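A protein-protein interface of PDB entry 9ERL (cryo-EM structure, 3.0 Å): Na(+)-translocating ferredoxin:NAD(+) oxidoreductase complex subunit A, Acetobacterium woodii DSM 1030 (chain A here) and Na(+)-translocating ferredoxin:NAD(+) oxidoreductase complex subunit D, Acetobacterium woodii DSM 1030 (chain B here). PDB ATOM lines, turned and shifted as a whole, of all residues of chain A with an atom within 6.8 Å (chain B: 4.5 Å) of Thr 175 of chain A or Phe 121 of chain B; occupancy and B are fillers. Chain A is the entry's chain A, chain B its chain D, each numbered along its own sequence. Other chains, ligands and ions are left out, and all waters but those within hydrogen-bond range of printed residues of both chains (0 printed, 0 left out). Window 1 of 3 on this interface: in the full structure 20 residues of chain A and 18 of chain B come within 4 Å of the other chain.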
ATOM      1  N   LEU A  18      18.895  32.053  29.012  1.00  0.00           N
ATOM      2  CA  LEU A  18      20.170  32.277  28.344  1.00  0.00           C
ATOM      3  C   LEU A  18      21.200  32.975  29.220  1.00  0.00           C
ATOM      4  O   LEU A  18      22.364  33.071  28.814  1.00  0.00           O
ATOM      5  CB  LEU A  18      19.944  33.082  27.062  1.00  0.00           C
ATOM      6  CG  LEU A  18      19.244  32.324  25.931  1.00  0.00           C
ATOM      7  CD1 LEU A  18      19.169  33.169  24.678  1.00  0.00           C
ATOM      8  CD2 LEU A  18      19.946  31.006  25.645  1.00  0.00           C
ATOM      9  N   PHE A 150      14.232  28.877  19.823  1.00  0.00           N
ATOM     10  CA  PHE A 150      14.986  27.629  19.714  1.00  0.00           C
ATOM     11  C   PHE A 150      14.270  26.616  18.828  1.00  0.00           C
ATOM     12  O   PHE A 150      14.905  25.942  18.003  1.00  0.00           O
ATOM     13  CB  PHE A 150      15.227  27.045  21.104  1.00  0.00           C
ATOM     14  CG  PHE A 150      16.360  26.063  21.164  1.00  0.00           C
ATOM     15  CD1 PHE A 150      17.443  26.180  20.312  1.00  0.00           C
ATOM     16  CD2 PHE A 150      16.340  25.022  22.075  1.00  0.00           C
ATOM     17  CE1 PHE A 150      18.483  25.277  20.369  1.00  0.00           C
ATOM     18  CE2 PHE A 150      17.378  24.118  22.135  1.00  0.00           C
ATOM     19  CZ  PHE A 150      18.450  24.245  21.281  1.00  0.00           C
ATOM     20  N   ILE A 153      14.684  27.600  15.180  1.00  0.00           N
ATOM     21  CA  ILE A 153      16.030  27.326  14.675  1.00  0.00           C
ATOM     22  C   ILE A 153      16.218  25.834  14.421  1.00  0.00           C
ATOM     23  O   ILE A 153      16.832  25.433  13.424  1.00  0.00           O
ATOM     24  CB  ILE A 153      17.093  27.880  15.642  1.00  0.00           C
ATOM     25  CG1 ILE A 153      17.079  29.407  15.637  1.00  0.00           C
ATOM     26  CG2 ILE A 153      18.474  27.390  15.263  1.00  0.00           C
ATOM     27  CD1 ILE A 153      17.653  30.018  16.886  1.00  0.00           C
ATOM     28  N   ARG A 154      15.695  24.986  15.312  1.00  0.00           N
ATOM     29  CA  ARG A 154      15.808  23.542  15.106  1.00  0.00           C
ATOM     30  C   ARG A 154      15.032  23.086  13.871  1.00  0.00           C
ATOM     31  O   ARG A 154      15.510  22.237  13.102  1.00  0.00           O
ATOM     32  CB  ARG A 154      15.332  22.799  16.352  1.00  0.00           C
ATOM     33  CG  ARG A 154      16.296  22.886  17.521  1.00  0.00           C
ATOM     34  CD  ARG A 154      15.825  22.043  18.691  1.00  0.00           C
ATOM     35  NE  ARG A 154      16.395  20.701  18.665  1.00  0.00           N
ATOM     36  CZ  ARG A 154      16.321  19.838  19.669  1.00  0.00           C
ATOM     37  NH1 ARG A 154      15.707  20.142  20.799  1.00  0.00           N
ATOM     38  NH2 ARG A 154      16.877  18.638  19.533  1.00  0.00           N
ATOM     39  N   ARG A 156      14.507  24.880  11.253  1.00  0.00           N
ATOM     40  CA  ARG A 156      15.355  25.275  10.128  1.00  0.00           C
ATOM     41  C   ARG A 156      16.505  24.293   9.923  1.00  0.00           C
ATOM     42  O   ARG A 156      16.802  23.903   8.788  1.00  0.00           O
ATOM     43  CB  ARG A 156      15.886  26.694  10.344  1.00  0.00           C
ATOM     44  CG  ARG A 156      17.266  26.966   9.750  1.00  0.00           C
ATOM     45  CD  ARG A 156      17.207  27.244   8.256  1.00  0.00           C
ATOM     46  NE  ARG A 156      18.480  26.968   7.602  1.00  0.00           N
ATOM     47  CZ  ARG A 156      19.372  27.893   7.275  1.00  0.00           C
ATOM     48  NH1 ARG A 156      19.160  29.175   7.520  1.00  0.00           N
ATOM     49  NH2 ARG A 156      20.503  27.524   6.684  1.00  0.00           N
ATOM     50  N   LEU A 157      17.156  23.872  11.011  1.00  0.00           N
ATOM     51  CA  LEU A 157      18.298  22.965  10.924  1.00  0.00           C
ATOM     52  C   LEU A 157      17.907  21.552  10.523  1.00  0.00           C
ATOM     53  O   LEU A 157      18.796  20.733  10.273  1.00  0.00           O
ATOM     54  CB  LEU A 157      19.043  22.913  12.258  1.00  0.00           C
ATOM     55  CG  LEU A 157      20.063  24.007  12.563  1.00  0.00           C
ATOM     56  CD1 LEU A 157      20.842  23.641  13.811  1.00  0.00           C
ATOM     57  CD2 LEU A 157      20.996  24.225  11.385  1.00  0.00           C
ATOM     58  N   SER A 160      19.694  20.334   7.274  1.00  0.00           N
ATOM     59  CA  SER A 160      21.131  20.543   7.212  1.00  0.00           C
ATOM     60  C   SER A 160      21.849  19.211   7.384  1.00  0.00           C
ATOM     61  O   SER A 160      21.300  18.252   7.933  1.00  0.00           O
ATOM     62  CB  SER A 160      21.603  21.537   8.279  1.00  0.00           C
ATOM     63  OG  SER A 160      21.334  22.871   7.889  1.00  0.00           O
ATOM     64  N   PRO A 170      24.352  17.351  20.978  1.00  0.00           N
ATOM     65  CA  PRO A 170      25.492  18.249  20.707  1.00  0.00           C
ATOM     66  C   PRO A 170      25.144  19.470  19.869  1.00  0.00           C
ATOM     67  O   PRO A 170      25.604  20.577  20.185  1.00  0.00           O
ATOM     68  CB  PRO A 170      26.485  17.331  19.985  1.00  0.00           C
ATOM     69  CG  PRO A 170      26.216  16.006  20.549  1.00  0.00           C
ATOM     70  CD  PRO A 170      24.733  15.944  20.735  1.00  0.00           C
ATOM     71  N   ILE A 171      24.326  19.319  18.824  1.00  0.00           N
ATOM     72  CA  ILE A 171      24.007  20.487  18.010  1.00  0.00           C
ATOM     73  C   ILE A 171      23.036  21.403  18.748  1.00  0.00           C
ATOM     74  O   ILE A 171      23.077  22.627  18.567  1.00  0.00           O
ATOM     75  CB  ILE A 171      23.491  20.068  16.618  1.00  0.00           C
ATOM     76  CG1 ILE A 171      24.117  20.952  15.541  1.00  0.00           C
ATOM     77  CG2 ILE A 171      21.976  20.173  16.516  1.00  0.00           C
ATOM     78  CD1 ILE A 171      25.566  20.644  15.263  1.00  0.00           C
ATOM     79  N   ALA A 172      22.188  20.849  19.624  1.00  0.00           N
ATOM     80  CA  ALA A 172      21.344  21.696  20.458  1.00  0.00           C
ATOM     81  C   ALA A 172      22.183  22.532  21.415  1.00  0.00           C
ATOM     82  O   ALA A 172      21.917  23.724  21.608  1.00  0.00           O
ATOM     83  CB  ALA A 172      20.338  20.843  21.226  1.00  0.00           C
ATOM     84  N   LEU A 173      23.215  21.927  22.007  1.00  0.00           N
ATOM     85  CA  LEU A 173      24.078  22.667  22.923  1.00  0.00           C
ATOM     86  C   LEU A 173      24.895  23.730  22.189  1.00  0.00           C
ATOM     87  O   LEU A 173      25.074  24.842  22.701  1.00  0.00           O
ATOM     88  CB  LEU A 173      24.984  21.699  23.682  1.00  0.00           C
ATOM     89  CG  LEU A 173      24.251  20.815  24.697  1.00  0.00           C
ATOM     90  CD1 LEU A 173      24.965  19.489  24.895  1.00  0.00           C
ATOM     91  CD2 LEU A 173      24.077  21.531  26.025  1.00  0.00           C
ATOM     92  N   LEU A 174      25.387  23.416  20.986  1.00  0.00           N
ATOM     93  CA  LEU A 174      26.119  24.420  20.211  1.00  0.00           C
ATOM     94  C   LEU A 174      25.216  25.585  19.805  1.00  0.00           C
ATOM     95  O   LEU A 174      25.629  26.754  19.866  1.00  0.00           O
ATOM     96  CB  LEU A 174      26.755  23.777  18.980  1.00  0.00           C
ATOM     97  CG  LEU A 174      27.863  22.747  19.220  1.00  0.00           C
ATOM     98  CD1 LEU A 174      27.992  21.811  18.032  1.00  0.00           C
ATOM     99  CD2 LEU A 174      29.189  23.426  19.506  1.00  0.00           C
ATOM    100  N   THR A 175      23.979  25.286  19.392  1.00  0.00           N
ATOM    101  CA  THR A 175      23.027  26.340  19.059  1.00  0.00           C
ATOM    102  C   THR A 175      22.712  27.207  20.271  1.00  0.00           C
ATOM    103  O   THR A 175      22.622  28.438  20.162  1.00  0.00           O
ATOM    104  CB  THR A 175      21.747  25.719  18.500  1.00  0.00           C
ATOM    105  OG1 THR A 175      22.073  24.846  17.413  1.00  0.00           O
ATOM    106  CG2 THR A 175      20.803  26.796  18.009  1.00  0.00           C
ATOM    107  N   ALA A 176      22.545  26.580  21.440  1.00  0.00           N
ATOM    108  CA  ALA A 176      22.297  27.337  22.661  1.00  0.00           C
ATOM    109  C   ALA A 176      23.481  28.232  23.007  1.00  0.00           C
ATOM    110  O   ALA A 176      23.295  29.360  23.474  1.00  0.00           O
ATOM    111  CB  ALA A 176      21.983  26.386  23.813  1.00  0.00           C
ATOM    112  N   GLY A 177      24.705  27.751  22.780  1.00  0.00           N
ATOM    113  CA  GLY A 177      25.874  28.584  23.028  1.00  0.00           C
ATOM    114  C   GLY A 177      25.946  29.795  22.113  1.00  0.00           C
ATOM    115  O   GLY A 177      26.290  30.899  22.550  1.00  0.00           O
ATOM    116  N   LEU A 178      25.625  29.606  20.830  1.00  0.00           N
ATOM    117  CA  LEU A 178      25.616  30.741  19.905  1.00  0.00           C
ATOM    118  C   LEU A 178      24.534  31.758  20.271  1.00  0.00           C
ATOM    119  O   LEU A 178      24.771  32.977  20.230  1.00  0.00           O
ATOM    120  CB  LEU A 178      25.440  30.246  18.471  1.00  0.00           C
ATOM    121  CG  LEU A 178      26.560  29.343  17.951  1.00  0.00           C
ATOM    122  CD1 LEU A 178      26.246  28.835  16.555  1.00  0.00           C
ATOM    123  CD2 LEU A 178      27.894  30.068  17.968  1.00  0.00           C
ATOM    124  N   MET A 179      23.342  31.278  20.644  1.00  0.00           N
ATOM    125  CA  MET A 179      22.290  32.182  21.103  1.00  0.00           C
ATOM    126  C   MET A 179      22.706  32.916  22.373  1.00  0.00           C
ATOM    127  O   MET A 179      22.384  34.099  22.554  1.00  0.00           O
ATOM    128  CB  MET A 179      20.996  31.405  21.339  1.00  0.00           C
ATOM    129  CG  MET A 179      20.337  30.876  20.080  1.00  0.00           C
ATOM    130  SD  MET A 179      18.910  29.838  20.444  1.00  0.00           S
ATOM    131  CE  MET A 179      17.779  31.043  21.131  1.00  0.00           C
ATOM    132  N   ALA A 180      23.420  32.228  23.269  1.00  0.00           N
ATOM    133  CA  ALA A 180      23.905  32.859  24.489  1.00  0.00           C
ATOM    134  C   ALA A 180      24.924  33.950  24.196  1.00  0.00           C
ATOM    135  O   ALA A 180      24.941  34.968  24.887  1.00  0.00           O
ATOM    136  CB  ALA A 180      24.502  31.808  25.422  1.00  0.00           C
ATOM    137  N   PHE B 114      28.245  22.288  11.248  1.00  0.00           N
ATOM    138  CA  PHE B 114      26.846  22.247  10.851  1.00  0.00           C
ATOM    139  C   PHE B 114      26.636  21.620   9.481  1.00  0.00           C
ATOM    140  O   PHE B 114      25.487  21.438   9.069  1.00  0.00           O
ATOM    141  CB  PHE B 114      26.251  23.659  10.868  1.00  0.00           C
ATOM    142  CG  PHE B 114      25.946  24.172  12.246  1.00  0.00           C
ATOM    143  CD1 PHE B 114      26.948  24.699  13.041  1.00  0.00           C
ATOM    144  CD2 PHE B 114      24.656  24.125  12.746  1.00  0.00           C
ATOM    145  CE1 PHE B 114      26.670  25.170  14.309  1.00  0.00           C
ATOM    146  CE2 PHE B 114      24.373  24.594  14.012  1.00  0.00           C
ATOM    147  CZ  PHE B 114      25.381  25.117  14.794  1.00  0.00           C
ATOM    148  N   GLN B 119      25.068  25.704   5.139  1.00  0.00           N
ATOM    149  CA  GLN B 119      24.296  24.894   6.070  1.00  0.00           C
ATOM    150  C   GLN B 119      24.210  25.491   7.467  1.00  0.00           C
ATOM    151  O   GLN B 119      23.544  24.910   8.330  1.00  0.00           O
ATOM    152  CB  GLN B 119      24.882  23.480   6.154  1.00  0.00           C
ATOM    153  CG  GLN B 119      25.401  22.941   4.836  1.00  0.00           C
ATOM    154  CD  GLN B 119      24.332  22.233   4.034  1.00  0.00           C
ATOM    155  OE1 GLN B 119      23.875  21.156   4.405  1.00  0.00           O
ATOM    156  NE2 GLN B 119      23.928  22.837   2.924  1.00  0.00           N
ATOM    157  N   ASN B 120      24.851  26.627   7.716  1.00  0.00           N
ATOM    158  CA  ASN B 120      24.785  27.284   9.012  1.00  0.00           C
ATOM    159  C   ASN B 120      23.673  28.328   9.019  1.00  0.00           C
ATOM    160  O   ASN B 120      23.094  28.664   7.985  1.00  0.00           O
ATOM    161  CB  ASN B 120      26.129  27.929   9.369  1.00  0.00           C
ATOM    162  CG  ASN B 120      26.633  28.866   8.292  1.00  0.00           C
ATOM    163  OD1 ASN B 120      26.103  28.905   7.185  1.00  0.00           O
ATOM    164  ND2 ASN B 120      27.658  29.640   8.620  1.00  0.00           N
ATOM    165  N   PHE B 121      23.378  28.841  10.211  1.00  0.00           N
ATOM    166  CA  PHE B 121      22.338  29.846  10.378  1.00  0.00           C
ATOM    167  C   PHE B 121      22.848  31.165  10.938  1.00  0.00           C
ATOM    168  O   PHE B 121      22.043  32.081  11.140  1.00  0.00           O
ATOM    169  CB  PHE B 121      21.212  29.304  11.275  1.00  0.00           C
ATOM    170  CG  PHE B 121      21.558  29.262  12.741  1.00  0.00           C
ATOM    171  CD1 PHE B 121      22.372  28.262  13.250  1.00  0.00           C
ATOM    172  CD2 PHE B 121      21.055  30.215  13.615  1.00  0.00           C
ATOM    173  CE1 PHE B 121      22.686  28.220  14.595  1.00  0.00           C
ATOM    174  CE2 PHE B 121      21.369  30.177  14.960  1.00  0.00           C
ATOM    175  CZ  PHE B 121      22.184  29.179  15.449  1.00  0.00           C
ATOM    176  N   ILE B 122      24.151  31.298  11.189  1.00  0.00           N
ATOM    177  CA  ILE B 122      24.707  32.482  11.826  1.00  0.00           C
ATOM    178  C   ILE B 122      25.959  32.924  11.076  1.00  0.00           C
ATOM    179  O   ILE B 122      26.571  32.158  10.330  1.00  0.00           O
ATOM    180  CB  ILE B 122      25.007  32.236  13.325  1.00  0.00           C
ATOM    181  CG1 ILE B 122      24.682  33.481  14.153  1.00  0.00           C
ATOM    182  CG2 ILE B 122      26.442  31.779  13.543  1.00  0.00           C
ATOM    183  CD1 ILE B 122      24.527  33.206  15.626  1.00  0.00           C
ATOM    184  N   ALA B 251      23.433  32.780   3.656  1.00  0.00           N
ATOM    185  CA  ALA B 251      22.935  31.718   4.521  1.00  0.00           C
ATOM    186  C   ALA B 251      22.231  32.235   5.768  1.00  0.00           C
ATOM    187  O   ALA B 251      21.681  31.425   6.520  1.00  0.00           O
ATOM    188  CB  ALA B 251      24.082  30.794   4.927  1.00  0.00           C
ATOM    189  N   SER B 252      22.232  33.546   6.009  1.00  0.00           N
ATOM    190  CA  SER B 252      21.658  34.111   7.220  1.00  0.00           C
ATOM    191  C   SER B 252      20.514  35.087   6.977  1.00  0.00           C
ATOM    192  O   SER B 252      19.954  35.602   7.951  1.00  0.00           O
ATOM    193  CB  SER B 252      22.745  34.819   8.041  1.00  0.00           C
ATOM    194  OG  SER B 252      23.951  34.080   8.023  1.00  0.00           O
ATOM    195  N   ASN B 292      19.779  37.207  13.070  1.00  0.00           N
ATOM    196  CA  ASN B 292      20.021  35.877  12.529  1.00  0.00           C
ATOM    197  C   ASN B 292      19.305  34.793  13.321  1.00  0.00           C
ATOM    198  O   ASN B 292      19.149  33.677  12.817  1.00  0.00           O
ATOM    199  CB  ASN B 292      21.524  35.575  12.507  1.00  0.00           C
ATOM    200  CG  ASN B 292      22.267  36.396  11.479  1.00  0.00           C
ATOM    201  OD1 ASN B 292      21.662  37.053  10.637  1.00  0.00           O
ATOM    202  ND2 ASN B 292      23.590  36.362  11.543  1.00  0.00           N
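Printed residues of chain A that touch a printed residue of chain B: Arg 156, Leu 157, Ser 160, Ile 171 and Thr 175.
Hydrophobic or aromatic side chains of chain A within 4 Å of the printed part of chain B: Leu 157 and Ile 171.
Of the 8 printed residues of chain B, 5 touch a printed residue of chain A.
Hydrophobic or aromatic side chains of chain B that line the printed part of chain A: Phe 114 and Phe 121.
Along chain B the printed residues that touch a printed residue of chain A span positions 114 to 251.
Among the printed residues, 7 pairs touch across the chains.
The backbone carbonyl oxygen of Asn 120 of chain B sits at hydrogen-bond distance from the guanidinium group of Arg 156 of chain A.
OG of Ser 160 of chain A is in hydrogen-bond range of O of Gln 119 of chain B, 3.0 Å away.
Printed residues of chain B within 4 Å of Arg 156 of chain A: Asn 120 and Ala 251.
Printed residues of chain B within 4 Å of Ile 171 of chain A: Phe 114.
Of chain B, only Phe 121 comes within 4 Å of Thr 175 of chain A.
Printed residues of chain A within 4 Å of Asn 120 of chain B: Arg 156 (3.1 Å).
Phe 121 of chain B touches just one residue of chain A: Thr 175 (3.8 Å).
Printed residues of chain A within 4 Å of Ala 251 of chain B: Arg 156 (3.5 Å).
The nearest printed residue of chain A that does not touch Asn 120 of chain B is Ser 160 of chain A (5.1 Å).
Among the printed residues, merely in contact across the chains: Arg 156 of chain A with Ala 251 of chain B (3.5 Å), Leu 157 of chain A with Phe 114 of chain B (3.7 Å), Thr 175 of chain A with Phe 121 of chain B (3.8 Å), Ile 171 of chain A with Phe 114 of chain B (3.96 Å) and Ser 160 of chain A with Phe 114 of chain B (3.96 Å).
The backbone carbonyl oxygen of Ile 122 of chain B sits at hydrogen-bond distance from the side-chain amide nitrogen of Asn 120 of chain B.
OG1 of Thr 175 of chain A sits at hydrogen-bond distance from O of Ile 171 of chain A (2.7 Å).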
